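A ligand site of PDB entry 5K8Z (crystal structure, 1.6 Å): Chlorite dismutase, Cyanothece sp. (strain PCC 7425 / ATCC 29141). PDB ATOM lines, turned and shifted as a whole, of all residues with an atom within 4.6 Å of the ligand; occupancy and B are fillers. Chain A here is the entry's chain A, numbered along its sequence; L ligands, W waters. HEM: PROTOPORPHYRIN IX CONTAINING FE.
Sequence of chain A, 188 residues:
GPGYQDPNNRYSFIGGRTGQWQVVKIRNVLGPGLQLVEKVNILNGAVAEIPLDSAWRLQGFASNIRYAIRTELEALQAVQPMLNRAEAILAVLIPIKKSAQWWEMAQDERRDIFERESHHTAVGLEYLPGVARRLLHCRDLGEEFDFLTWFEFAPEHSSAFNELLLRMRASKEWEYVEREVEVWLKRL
A ring nitrogen (NE2) of His 120 binds an iron atom (FE) of the ligand, 2.3 Å away. An oxygen (O1A) of the ligand is in hydrogen-bond range of the backbone NH of Arg 66, 2.8 Å away. The side-chain amino group of Lys 98 is in salt-bridge range of an oxygen (O2D) of the ligand, at 2.7 Å. An oxygen (O2A) of the ligand sits at hydrogen-bond distance from the backbone NH (N) of Tyr 67 (2.9 Å). N of Ala 68 lies within hydrogen-bond range of O2A of the ligand (2.9 Å).
The guanidinium group (NE) of Arg 169 is in salt-bridge range of the side-chain carboxylate (OE2) of Glu 180, at 2.8 Å. NE1 of Trp 174 is in hydrogen-bond range of OE1 of Glu 180, at 2.9 Å. The backbone carbonyl oxygen (O) of Ile 94 sits at hydrogen-bond distance from the side-chain hydroxyl (OG1) of Thr 149, at 2.6 Å. O of Ile 96 is in hydrogen-bond range of N of Phe 147. The side-chain amino group (NZ) of Lys 98 is in salt-bridge range of the side-chain carboxylate (OE2) of Glu 173 (2.9 Å). The guanidinium group of Arg 66 lies within hydrogen-bond range of the backbone carbonyl oxygen of Asn 64, at 3.1 Å. The backbone carbonyl oxygen (O) of Phe 114 sits at hydrogen-bond distance from the backbone NH (N) of His 120. ND1 of His 120 lies within hydrogen-bond range of OE1 of Glu 173, 2.7 Å away.
Merely in contact with the ligand: Phe 151, Leu 164, Thr 121, Ile 65, Phe 147, Gly 124, Phe 114, Leu 165, Arg 133, Met 168, Trp 174, Ile 96, Leu 135, Leu 76, Trp 102, Ile 94, Leu 128, Thr 149, Val 131 and Glu 180. Hydrophobic or aromatic side chains that line the ligand: Ile 65, Tyr 67, Ala 68, Leu 76, Ile 94, Ile 96, Trp 102, Phe 114, His 120, Leu 128, Val 131, Leu 135, Phe 147, Phe 151, Leu 164, Leu 165, Met 168 and Trp 174. 25 residues have an atom within 4 Å of the ligand: Ile 65, Arg 66, Tyr 67, Ala 68, Leu 76, Ile 94, Ile 96, Lys 98, Trp 102, Phe 114, His 120, Thr 121, Gly 124, Leu 128, Val 131, Arg 133, Leu 135, Phe 147, Thr 149, Phe 151, Leu 164, Leu 165, Met 168, Trp 174 and Glu 180.
Water W1 lies within hydrogen-bond range of O2D of the ligand, OH of Tyr 67 and NE1 of Trp 102. Water W3 lies within hydrogen-bond range of O1A of the ligand (2.8 Å) and O of Asn 64 (2.8 Å).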
ATOM      1  N   ASN A  64      28.424  26.005  23.020  1.00  0.00           N
ATOM      2  CA  ASN A  64      28.796  25.452  24.315  1.00  0.00           C
ATOM      3  C   ASN A  64      28.428  23.969  24.409  1.00  0.00           C
ATOM      4  O   ASN A  64      27.576  23.446  23.661  1.00  0.00           O
ATOM      5  CB  ASN A  64      28.115  26.225  25.450  1.00  0.00           C
ATOM      6  CG  ASN A  64      26.591  26.203  25.352  1.00  0.00           C
ATOM      7  OD1 ASN A  64      26.000  26.948  24.563  1.00  0.00           O
ATOM      8  ND2 ASN A  64      25.963  25.349  26.149  1.00  0.00           N
ATOM      9  N   ILE A  65      29.069  23.287  25.358  1.00  0.00           N
ATOM     10  CA  ILE A  65      28.795  21.888  25.632  1.00  0.00           C
ATOM     11  C   ILE A  65      27.341  21.701  26.065  1.00  0.00           C
ATOM     12  O   ILE A  65      26.792  22.486  26.847  1.00  0.00           O
ATOM     13  CB  ILE A  65      29.788  21.394  26.706  1.00  0.00           C
ATOM     14  CG1 ILE A  65      31.202  21.281  26.111  1.00  0.00           C
ATOM     15  CG2 ILE A  65      29.352  20.081  27.315  1.00  0.00           C
ATOM     16  CD1 ILE A  65      31.379  20.176  25.069  1.00  0.00           C
ATOM     17  N   ARG A  66      26.716  20.629  25.554  1.00  0.00           N
ATOM     18  CA  ARG A  66      25.306  20.319  25.818  1.00  0.00           C
ATOM     19  C   ARG A  66      25.080  19.045  26.624  1.00  0.00           C
ATOM     20  O   ARG A  66      24.038  18.916  27.261  1.00  0.00           O
ATOM     21  CB  ARG A  66      24.541  20.157  24.487  1.00  0.00           C
ATOM     22  CG  ARG A  66      24.712  21.289  23.490  1.00  0.00           C
ATOM     23  CD  ARG A  66      24.339  22.641  24.087  1.00  0.00           C
ATOM     24  NE  ARG A  66      24.530  23.736  23.132  1.00  0.00           N
ATOM     25  CZ  ARG A  66      23.646  24.078  22.193  1.00  0.00           C
ATOM     26  NH1 ARG A  66      22.485  23.440  22.094  1.00  0.00           N
ATOM     27  NH2 ARG A  66      23.922  25.077  21.367  1.00  0.00           N
ATOM     28  N   TYR A  67      26.019  18.089  26.592  1.00  0.00           N
ATOM     29  CA  TYR A  67      25.837  16.793  27.263  1.00  0.00           C
ATOM     30  C   TYR A  67      27.042  16.352  28.066  1.00  0.00           C
ATOM     31  O   TYR A  67      26.879  15.766  29.139  1.00  0.00           O
ATOM     32  CB  TYR A  67      25.473  15.696  26.219  1.00  0.00           C
ATOM     33  CG  TYR A  67      24.149  15.940  25.540  1.00  0.00           C
ATOM     34  CD1 TYR A  67      22.955  15.798  26.240  1.00  0.00           C
ATOM     35  CD2 TYR A  67      24.080  16.331  24.205  1.00  0.00           C
ATOM     36  CE1 TYR A  67      21.730  16.029  25.631  1.00  0.00           C
ATOM     37  CE2 TYR A  67      22.863  16.571  23.584  1.00  0.00           C
ATOM     38  CZ  TYR A  67      21.688  16.424  24.308  1.00  0.00           C
ATOM     39  OH  TYR A  67      20.477  16.661  23.705  1.00  0.00           O
ATOM     40  N   ALA A  68      28.263  16.610  27.585  1.00  0.00           N
ATOM     41  CA  ALA A  68      29.450  16.059  28.221  1.00  0.00           C
ATOM     42  C   ALA A  68      29.623  16.602  29.636  1.00  0.00           C
ATOM     43  O   ALA A  68      29.464  17.806  29.895  1.00  0.00           O
ATOM     44  CB  ALA A  68      30.696  16.380  27.397  1.00  0.00           C
ATOM     45  N   LEU A  76      38.554  13.653  27.302  1.00  0.00           N
ATOM     46  CA  LEU A  76      38.679  14.089  25.915  1.00  0.00           C
ATOM     47  C   LEU A  76      39.892  14.997  25.730  1.00  0.00           C
ATOM     48  O   LEU A  76      40.694  14.811  24.807  1.00  0.00           O
ATOM     49  CB  LEU A  76      37.402  14.801  25.480  1.00  0.00           C
ATOM     50  CG  LEU A  76      36.182  13.884  25.303  1.00  0.00           C
ATOM     51  CD1 LEU A  76      34.890  14.660  25.436  1.00  0.00           C
ATOM     52  CD2 LEU A  76      36.245  13.207  23.948  1.00  0.00           C
ATOM     53  N   ILE A  94      29.824  15.566   7.736  1.00  0.00           N
ATOM     54  CA  ILE A  94      28.633  14.727   7.889  1.00  0.00           C
ATOM     55  C   ILE A  94      27.491  15.553   8.456  1.00  0.00           C
ATOM     56  O   ILE A  94      27.351  15.659   9.681  1.00  0.00           O
ATOM     57  CB  ILE A  94      28.927  13.487   8.763  1.00  0.00           C
ATOM     58  CG1 ILE A  94      30.150  12.735   8.230  1.00  0.00           C
ATOM     59  CG2 ILE A  94      27.700  12.569   8.801  1.00  0.00           C
ATOM     60  CD1 ILE A  94      30.503  11.458   8.993  1.00  0.00           C
ATOM     61  N   ILE A  96      23.739  16.168   9.708  1.00  0.00           N
ATOM     62  CA  ILE A  96      22.864  15.225  10.410  1.00  0.00           C
ATOM     63  C   ILE A  96      21.612  15.956  10.876  1.00  0.00           C
ATOM     64  O   ILE A  96      21.687  17.078  11.394  1.00  0.00           O
ATOM     65  CB  ILE A  96      23.603  14.602  11.621  1.00  0.00           C
ATOM     66  CG1 ILE A  96      24.640  13.579  11.130  1.00  0.00           C
ATOM     67  CG2 ILE A  96      22.608  13.965  12.605  1.00  0.00           C
ATOM     68  CD1 ILE A  96      25.553  13.061  12.207  1.00  0.00           C
ATOM     69  N   LYS A  98      18.079  15.190  13.246  1.00  0.00           N
ATOM     70  CA  LYS A  98      17.372  14.323  14.186  1.00  0.00           C
ATOM     71  C   LYS A  98      15.879  14.639  14.151  1.00  0.00           C
ATOM     72  O   LYS A  98      15.464  15.708  13.704  1.00  0.00           O
ATOM     73  CB  LYS A  98      17.922  14.494  15.605  1.00  0.00           C
ATOM     74  CG  LYS A  98      19.335  13.921  15.785  1.00  0.00           C
ATOM     75  CD  LYS A  98      19.793  13.965  17.251  1.00  0.00           C
ATOM     76  CE  LYS A  98      21.177  13.327  17.413  1.00  0.00           C
ATOM     77  NZ  LYS A  98      21.644  13.250  18.818  1.00  0.00           N
ATOM     78  N   TRP A 102      12.993  13.427  18.971  1.00  0.00           N
ATOM     79  CA  TRP A 102      14.198  13.682  19.753  1.00  0.00           C
ATOM     80  C   TRP A 102      14.137  15.049  20.425  1.00  0.00           C
ATOM     81  O   TRP A 102      14.385  15.180  21.634  1.00  0.00           O
ATOM     82  CB  TRP A 102      15.430  13.591  18.862  1.00  0.00           C
ATOM     83  CG  TRP A 102      16.698  14.075  19.524  1.00  0.00           C
ATOM     84  CD1 TRP A 102      17.268  15.304  19.402  1.00  0.00           C
ATOM     85  CD2 TRP A 102      17.526  13.338  20.422  1.00  0.00           C
ATOM     86  NE1 TRP A 102      18.410  15.379  20.163  1.00  0.00           N
ATOM     87  CE2 TRP A 102      18.591  14.174  20.804  1.00  0.00           C
ATOM     88  CE3 TRP A 102      17.473  12.033  20.951  1.00  0.00           C
ATOM     89  CZ2 TRP A 102      19.598  13.770  21.670  1.00  0.00           C
ATOM     90  CZ3 TRP A 102      18.468  11.632  21.811  1.00  0.00           C
ATOM     91  CH2 TRP A 102      19.527  12.491  22.165  1.00  0.00           C
ATOM     92  N   PHE A 114      21.955   9.557  24.833  1.00  0.00           N
ATOM     93  CA  PHE A 114      23.232   9.932  24.240  1.00  0.00           C
ATOM     94  C   PHE A 114      24.385   9.125  24.824  1.00  0.00           C
ATOM     95  O   PHE A 114      25.223   8.595  24.080  1.00  0.00           O
ATOM     96  CB  PHE A 114      23.468  11.436  24.451  1.00  0.00           C
ATOM     97  CG  PHE A 114      24.781  11.934  23.893  1.00  0.00           C
ATOM     98  CD1 PHE A 114      24.907  12.225  22.551  1.00  0.00           C
ATOM     99  CD2 PHE A 114      25.870  12.148  24.733  1.00  0.00           C
ATOM    100  CE1 PHE A 114      26.094  12.716  22.036  1.00  0.00           C
ATOM    101  CE2 PHE A 114      27.066  12.638  24.214  1.00  0.00           C
ATOM    102  CZ  PHE A 114      27.179  12.910  22.875  1.00  0.00           C
ATOM    103  N   HIS A 120      28.079   7.400  23.528  1.00  0.00           N
ATOM    104  CA  HIS A 120      28.619   8.166  22.421  1.00  0.00           C
ATOM    105  C   HIS A 120      30.057   8.616  22.687  1.00  0.00           C
ATOM    106  O   HIS A 120      30.957   8.405  21.865  1.00  0.00           O
ATOM    107  CB  HIS A 120      27.719   9.365  22.149  1.00  0.00           C
ATOM    108  CG  HIS A 120      28.109  10.156  20.947  1.00  0.00           C
ATOM    109  ND1 HIS A 120      27.235  10.429  19.922  1.00  0.00           N
ATOM    110  CD2 HIS A 120      29.275  10.755  20.613  1.00  0.00           C
ATOM    111  CE1 HIS A 120      27.851  11.160  19.007  1.00  0.00           C
ATOM    112  NE2 HIS A 120      29.085  11.358  19.400  1.00  0.00           N
ATOM    113  N   THR A 121      30.291   9.242  23.846  1.00  0.00           N
ATOM    114  CA  THR A 121      31.641   9.728  24.148  1.00  0.00           C
ATOM    115  C   THR A 121      32.608   8.578  24.402  1.00  0.00           C
ATOM    116  O   THR A 121      33.770   8.630  23.980  1.00  0.00           O
ATOM    117  CB  THR A 121      31.592  10.676  25.350  1.00  0.00           C
ATOM    118  OG1 THR A 121      30.776  11.800  25.018  1.00  0.00           O
ATOM    119  CG2 THR A 121      32.998  11.157  25.717  1.00  0.00           C
ATOM    120  N   GLY A 124      33.516   7.047  21.088  1.00  0.00           N
ATOM    121  CA  GLY A 124      34.335   7.992  20.353  1.00  0.00           C
ATOM    122  C   GLY A 124      35.756   8.074  20.868  1.00  0.00           C
ATOM    123  O   GLY A 124      36.704   8.158  20.087  1.00  0.00           O
ATOM    124  N   LEU A 125      35.922   8.052  22.194  1.00  0.00           N
ATOM    125  CA  LEU A 125      37.258   8.159  22.763  1.00  0.00           C
ATOM    126  C   LEU A 125      38.205   7.075  22.232  1.00  0.00           C
ATOM    127  O   LEU A 125      39.414   7.302  22.168  1.00  0.00           O
ATOM    128  CB  LEU A 125      37.197   8.080  24.290  1.00  0.00           C
ATOM    129  CG  LEU A 125      36.981   9.392  25.040  1.00  0.00           C
ATOM    130  CD1 LEU A 125      36.628   9.111  26.495  1.00  0.00           C
ATOM    131  CD2 LEU A 125      38.216  10.280  24.953  1.00  0.00           C
ATOM    132  N   LEU A 128      40.488   8.258  19.296  1.00  0.00           N
ATOM    133  CA  LEU A 128      41.443   9.330  19.500  1.00  0.00           C
ATOM    134  C   LEU A 128      42.785   8.748  19.928  1.00  0.00           C
ATOM    135  O   LEU A 128      42.825   7.694  20.583  1.00  0.00           O
ATOM    136  CB  LEU A 128      40.938  10.306  20.566  1.00  0.00           C
ATOM    137  CG  LEU A 128      39.912  11.356  20.118  1.00  0.00           C
ATOM    138  CD1 LEU A 128      38.826  10.765  19.240  1.00  0.00           C
ATOM    139  CD2 LEU A 128      39.288  12.042  21.328  1.00  0.00           C
ATOM    140  N   VAL A 131      41.653  10.528  15.179  1.00  0.00           N
ATOM    141  CA  VAL A 131      40.608  11.316  14.545  1.00  0.00           C
ATOM    142  C   VAL A 131      40.443  12.639  15.279  1.00  0.00           C
ATOM    143  O   VAL A 131      40.217  12.661  16.492  1.00  0.00           O
ATOM    144  CB  VAL A 131      39.271  10.546  14.534  1.00  0.00           C
ATOM    145  CG1 VAL A 131      38.157  11.379  13.897  1.00  0.00           C
ATOM    146  CG2 VAL A 131      39.414   9.207  13.805  1.00  0.00           C
ATOM    147  N   ARG A 133      38.079  16.230  15.391  1.00  0.00           N
ATOM    148  CA  ARG A 133      36.656  16.491  15.165  1.00  0.00           C
ATOM    149  C   ARG A 133      36.313  17.944  15.476  1.00  0.00           C
ATOM    150  O   ARG A 133      37.003  18.622  16.236  1.00  0.00           O
ATOM    151  CB  ARG A 133      35.772  15.563  16.010  1.00  0.00           C
ATOM    152  CG  ARG A 133      35.751  15.918  17.491  1.00  0.00           C
ATOM    153  CD  ARG A 133      34.929  14.948  18.320  1.00  0.00           C
ATOM    154  NE  ARG A 133      34.718  15.502  19.658  1.00  0.00           N
ATOM    155  CZ  ARG A 133      35.669  15.607  20.586  1.00  0.00           C
ATOM    156  NH1 ARG A 133      36.913  15.194  20.323  1.00  0.00           N
ATOM    157  NH2 ARG A 133      35.385  16.144  21.766  1.00  0.00           N
ATOM    158  N   LEU A 135      32.312  20.110  15.995  1.00  0.00           N
ATOM    159  CA  LEU A 135      30.866  20.002  16.062  1.00  0.00           C
ATOM    160  C   LEU A 135      30.261  21.381  15.880  1.00  0.00           C
ATOM    161  O   LEU A 135      30.582  22.297  16.639  1.00  0.00           O
ATOM    162  CB  LEU A 135      30.423  19.408  17.403  1.00  0.00           C
ATOM    163  CG  LEU A 135      28.920  19.432  17.687  1.00  0.00           C
ATOM    164  CD1 LEU A 135      28.161  18.652  16.618  1.00  0.00           C
ATOM    165  CD2 LEU A 135      28.630  18.866  19.073  1.00  0.00           C
ATOM    166  N   PHE A 147      22.920  19.451  12.601  1.00  0.00           N
ATOM    167  CA  PHE A 147      24.332  19.533  12.949  1.00  0.00           C
ATOM    168  C   PHE A 147      25.170  19.420  11.681  1.00  0.00           C
ATOM    169  O   PHE A 147      24.798  18.729  10.733  1.00  0.00           O
ATOM    170  CB  PHE A 147      24.764  18.434  13.920  1.00  0.00           C
ATOM    171  CG  PHE A 147      23.865  18.278  15.101  1.00  0.00           C
ATOM    172  CD1 PHE A 147      24.019  19.076  16.224  1.00  0.00           C
ATOM    173  CD2 PHE A 147      22.848  17.330  15.105  1.00  0.00           C
ATOM    174  CE1 PHE A 147      23.181  18.943  17.323  1.00  0.00           C
ATOM    175  CE2 PHE A 147      22.007  17.198  16.194  1.00  0.00           C
ATOM    176  CZ  PHE A 147      22.169  18.005  17.305  1.00  0.00           C
ATOM    177  N   THR A 149      28.844  18.036  11.352  1.00  0.00           N
ATOM    178  CA  THR A 149      29.956  17.396  12.035  1.00  0.00           C
ATOM    179  C   THR A 149      31.151  17.274  11.089  1.00  0.00           C
ATOM    180  O   THR A 149      30.986  17.076   9.874  1.00  0.00           O
ATOM    181  CB  THR A 149      29.556  16.027  12.592  1.00  0.00           C
ATOM    182  OG1 THR A 149      29.151  15.144  11.536  1.00  0.00           O
ATOM    183  CG2 THR A 149      28.394  16.180  13.584  1.00  0.00           C
ATOM    184  N   PHE A 151      35.304  15.791  10.612  1.00  0.00           N
ATOM    185  CA  PHE A 151      36.326  14.864  11.077  1.00  0.00           C
ATOM    186  C   PHE A 151      37.476  14.897  10.081  1.00  0.00           C
ATOM    187  O   PHE A 151      37.247  15.038   8.877  1.00  0.00           O
ATOM    188  CB  PHE A 151      35.764  13.448  11.226  1.00  0.00           C
ATOM    189  CG  PHE A 151      34.503  13.396  12.024  1.00  0.00           C
ATOM    190  CD1 PHE A 151      34.543  13.233  13.399  1.00  0.00           C
ATOM    191  CD2 PHE A 151      33.283  13.554  11.405  1.00  0.00           C
ATOM    192  CE1 PHE A 151      33.389  13.224  14.143  1.00  0.00           C
ATOM    193  CE2 PHE A 151      32.126  13.546  12.140  1.00  0.00           C
ATOM    194  CZ  PHE A 151      32.175  13.382  13.511  1.00  0.00           C
ATOM    195  N   PHE A 161      38.044   4.904  11.179  1.00  0.00           N
ATOM    196  CA  PHE A 161      36.911   5.822  11.114  1.00  0.00           C
ATOM    197  C   PHE A 161      35.691   5.132  10.507  1.00  0.00           C
ATOM    198  O   PHE A 161      34.554   5.349  10.953  1.00  0.00           O
ATOM    199  CB  PHE A 161      37.272   7.068  10.310  1.00  0.00           C
ATOM    200  CG  PHE A 161      36.200   8.105  10.292  1.00  0.00           C
ATOM    201  CD1 PHE A 161      35.983   8.907  11.407  1.00  0.00           C
ATOM    202  CD2 PHE A 161      35.393   8.277   9.178  1.00  0.00           C
ATOM    203  CE1 PHE A 161      34.989   9.866  11.405  1.00  0.00           C
ATOM    204  CE2 PHE A 161      34.391   9.247   9.180  1.00  0.00           C
ATOM    205  CZ  PHE A 161      34.204  10.033  10.293  1.00  0.00           C
ATOM    206  N   LEU A 164      34.184   3.217  13.272  1.00  0.00           N
ATOM    207  CA  LEU A 164      33.453   4.095  14.160  1.00  0.00           C
ATOM    208  C   LEU A 164      32.070   4.416  13.607  1.00  0.00           C
ATOM    209  O   LEU A 164      31.080   4.415  14.349  1.00  0.00           O
ATOM    210  CB  LEU A 164      34.270   5.378  14.385  1.00  0.00           C
ATOM    211  CG  LEU A 164      33.601   6.538  15.127  1.00  0.00           C
ATOM    212  CD1 LEU A 164      33.178   6.141  16.538  1.00  0.00           C
ATOM    213  CD2 LEU A 164      34.543   7.714  15.156  1.00  0.00           C
ATOM    214  N   LEU A 165      31.989   4.726  12.309  1.00  0.00           N
ATOM    215  CA  LEU A 165      30.696   5.031  11.711  1.00  0.00           C
ATOM    216  C   LEU A 165      29.748   3.846  11.875  1.00  0.00           C
ATOM    217  O   LEU A 165      28.584   4.011  12.272  1.00  0.00           O
ATOM    218  CB  LEU A 165      30.857   5.373  10.236  1.00  0.00           C
ATOM    219  CG  LEU A 165      31.545   6.692   9.892  1.00  0.00           C
ATOM    220  CD1 LEU A 165      31.689   6.824   8.385  1.00  0.00           C
ATOM    221  CD2 LEU A 165      30.764   7.883  10.463  1.00  0.00           C
ATOM    222  N   MET A 168      28.298   3.716  15.451  1.00  0.00           N
ATOM    223  CA  MET A 168      27.376   4.782  15.853  1.00  0.00           C
ATOM    224  C   MET A 168      26.044   4.641  15.139  1.00  0.00           C
ATOM    225  O   MET A 168      24.989   4.854  15.749  1.00  0.00           O
ATOM    226  CB  MET A 168      28.025   6.135  15.591  1.00  0.00           C
ATOM    227  CG  MET A 168      29.299   6.323  16.416  1.00  0.00           C
ATOM    228  SD  MET A 168      29.755   8.021  16.744  1.00  0.00           S
ATOM    229  CE  MET A 168      30.372   7.858  18.418  1.00  0.00           C
ATOM    230  N   ARG A 169      26.057   4.246  13.859  1.00  0.00           N
ATOM    231  CA  ARG A 169      24.811   4.089  13.123  1.00  0.00           C
ATOM    232  C   ARG A 169      23.931   2.981  13.689  1.00  0.00           C
ATOM    233  O   ARG A 169      22.739   2.913  13.373  1.00  0.00           O
ATOM    234  CB  ARG A 169      25.099   3.823  11.645  1.00  0.00           C
ATOM    235  CG  ARG A 169      25.233   5.088  10.774  1.00  0.00           C
ATOM    236  CD  ARG A 169      26.386   5.985  11.217  1.00  0.00           C
ATOM    237  NE  ARG A 169      26.602   7.113  10.311  1.00  0.00           N
ATOM    238  CZ  ARG A 169      27.277   7.036   9.169  1.00  0.00           C
ATOM    239  NH1 ARG A 169      27.780   5.882   8.764  1.00  0.00           N
ATOM    240  NH2 ARG A 169      27.433   8.117   8.416  1.00  0.00           N
ATOM    241  N   GLU A 173      20.917   6.136  19.907  1.00  0.00           N
ATOM    242  CA  GLU A 173      20.892   7.533  19.470  1.00  0.00           C
ATOM    243  C   GLU A 173      20.521   7.636  17.991  1.00  0.00           C
ATOM    244  O   GLU A 173      19.699   8.467  17.615  1.00  0.00           O
ATOM    245  CB  GLU A 173      22.263   8.181  19.721  1.00  0.00           C
ATOM    246  CG  GLU A 173      22.325   9.650  19.338  1.00  0.00           C
ATOM    247  CD  GLU A 173      23.710  10.240  19.480  1.00  0.00           C
ATOM    248  OE1 GLU A 173      24.661   9.478  19.789  1.00  0.00           O
ATOM    249  OE2 GLU A 173      23.865  11.465  19.290  1.00  0.00           O
ATOM    250  N   TRP A 174      21.114   6.783  17.155  1.00  0.00           N
ATOM    251  CA  TRP A 174      20.894   6.925  15.713  1.00  0.00           C
ATOM    252  C   TRP A 174      19.497   6.496  15.285  1.00  0.00           C
ATOM    253  O   TRP A 174      19.113   6.788  14.144  1.00  0.00           O
ATOM    254  CB  TRP A 174      21.955   6.127  14.943  1.00  0.00           C
ATOM    255  CG  TRP A 174      22.847   7.039  14.157  1.00  0.00           C
ATOM    256  CD1 TRP A 174      22.842   7.224  12.806  1.00  0.00           C
ATOM    257  CD2 TRP A 174      23.843   7.912  14.685  1.00  0.00           C
ATOM    258  NE1 TRP A 174      23.795   8.163  12.460  1.00  0.00           N
ATOM    259  CE2 TRP A 174      24.419   8.599  13.597  1.00  0.00           C
ATOM    260  CE3 TRP A 174      24.301   8.190  15.978  1.00  0.00           C
ATOM    261  CZ2 TRP A 174      25.433   9.538  13.764  1.00  0.00           C
ATOM    262  CZ3 TRP A 174      25.322   9.129  16.132  1.00  0.00           C
ATOM    263  CH2 TRP A 174      25.873   9.780  15.027  1.00  0.00           C
ATOM    264  N   GLU A 180      20.947  12.131   6.739  1.00  0.00           N
ATOM    265  CA  GLU A 180      22.383  12.032   6.949  1.00  0.00           C
ATOM    266  C   GLU A 180      23.095  11.897   5.616  1.00  0.00           C
ATOM    267  O   GLU A 180      22.662  11.132   4.744  1.00  0.00           O
ATOM    268  CB  GLU A 180      22.727  10.861   7.867  1.00  0.00           C
ATOM    269  CG  GLU A 180      24.159  10.832   8.322  1.00  0.00           C
ATOM    270  CD  GLU A 180      24.428   9.761   9.365  1.00  0.00           C
ATOM    271  OE1 GLU A 180      23.518   8.951   9.647  1.00  0.00           O
ATOM    272  OE2 GLU A 180      25.555   9.728   9.904  1.00  0.00           O
HETATM  273  CHA HEM L   1      28.186  15.274  19.913  1.00  0.00           C
HETATM  274  CHB HEM L   1      32.349  12.991  20.987  1.00  0.00           C
HETATM  275  CHC HEM L   1      32.409  10.967  16.543  1.00  0.00           C
HETATM  276  CHD HEM L   1      28.075  12.970  15.612  1.00  0.00           C
HETATM  277  C1A HEM L   1      29.295  14.839  20.602  1.00  0.00           C
HETATM  278  C2A HEM L   1      29.660  15.172  21.966  1.00  0.00           C
HETATM  279  C3A HEM L   1      30.803  14.536  22.265  1.00  0.00           C
HETATM  280  C4A HEM L   1      31.214  13.778  21.099  1.00  0.00           C
HETATM  281  CMA HEM L   1      31.562  14.586  23.606  1.00  0.00           C
HETATM  282  CAA HEM L   1      28.842  16.074  22.930  1.00  0.00           C
HETATM  283  CBA HEM L   1      29.229  17.543  22.839  1.00  0.00           C
HETATM  284  CGA HEM L   1      28.362  18.313  23.793  1.00  0.00           C
HETATM  285  O1A HEM L   1      27.643  19.249  23.350  1.00  0.00           O
HETATM  286  O2A HEM L   1      28.393  17.977  24.999  1.00  0.00           O
HETATM  287  C1B HEM L   1      32.755  12.315  19.854  1.00  0.00           C
HETATM  288  C2B HEM L   1      34.053  11.693  19.663  1.00  0.00           C
HETATM  289  C3B HEM L   1      34.094  11.157  18.441  1.00  0.00           C
HETATM  290  C4B HEM L   1      32.797  11.382  17.814  1.00  0.00           C
HETATM  291  CMB HEM L   1      35.214  11.689  20.685  1.00  0.00           C
HETATM  292  CAB HEM L   1      35.306  10.410  17.848  1.00  0.00           C
HETATM  293  CBB HEM L   1      35.533  10.444  16.525  1.00  0.00           C
HETATM  294  C1C HEM L   1      31.225  11.292  15.910  1.00  0.00           C
HETATM  295  C2C HEM L   1      30.784  10.827  14.609  1.00  0.00           C
HETATM  296  C3C HEM L   1      29.582  11.393  14.333  1.00  0.00           C
HETATM  297  C4C HEM L   1      29.228  12.212  15.476  1.00  0.00           C
HETATM  298  CMC HEM L   1      31.662   9.877  13.746  1.00  0.00           C
HETATM  299  CAC HEM L   1      28.648  11.270  13.109  1.00  0.00           C
HETATM  300  CBC HEM L   1      28.745  10.351  12.139  1.00  0.00           C
HETATM  301  C1D HEM L   1      27.736  13.800  16.677  1.00  0.00           C
HETATM  302  C2D HEM L   1      26.546  14.620  16.769  1.00  0.00           C
HETATM  303  C3D HEM L   1      26.582  15.255  17.945  1.00  0.00           C
HETATM  304  C4D HEM L   1      27.781  14.851  18.659  1.00  0.00           C
HETATM  305  CMD HEM L   1      25.456  14.746  15.673  1.00  0.00           C
HETATM  306  CAD HEM L   1      25.532  16.236  18.509  1.00  0.00           C
HETATM  307  CBD HEM L   1      24.610  15.415  19.403  1.00  0.00           C
HETATM  308  CGD HEM L   1      23.429  16.223  19.874  1.00  0.00           C
HETATM  309  O1D HEM L   1      23.602  17.403  20.280  1.00  0.00           O
HETATM  310  O2D HEM L   1      22.297  15.667  19.871  1.00  0.00           O
HETATM  311  NA  HEM L   1      30.279  14.000  20.110  1.00  0.00           N
HETATM  312  NB  HEM L   1      32.009  12.108  18.713  1.00  0.00           N
HETATM  313  NC  HEM L   1      30.239  12.120  16.401  1.00  0.00           N
HETATM  314  ND  HEM L   1      28.451  13.961  17.844  1.00  0.00           N
HETATM  315 FE   HEM L   1      30.213  12.997  18.280  1.00  0.00          FE
HETATM  316  O   HOH W   1      20.478  17.230  21.077  1.00  0.00           O
HETATM  317  O   HOH W   2      25.722  18.733  21.186  1.00  0.00           O
HETATM  318  O   HOH W   3      28.136  21.485  21.685  1.00  0.00           O
HETATM  319  O   HOH W   4      32.196  16.709  19.678  1.00  0.00           O
HETATM  320  O   HOH W   5      22.020  19.593  21.086  1.00  0.00           O
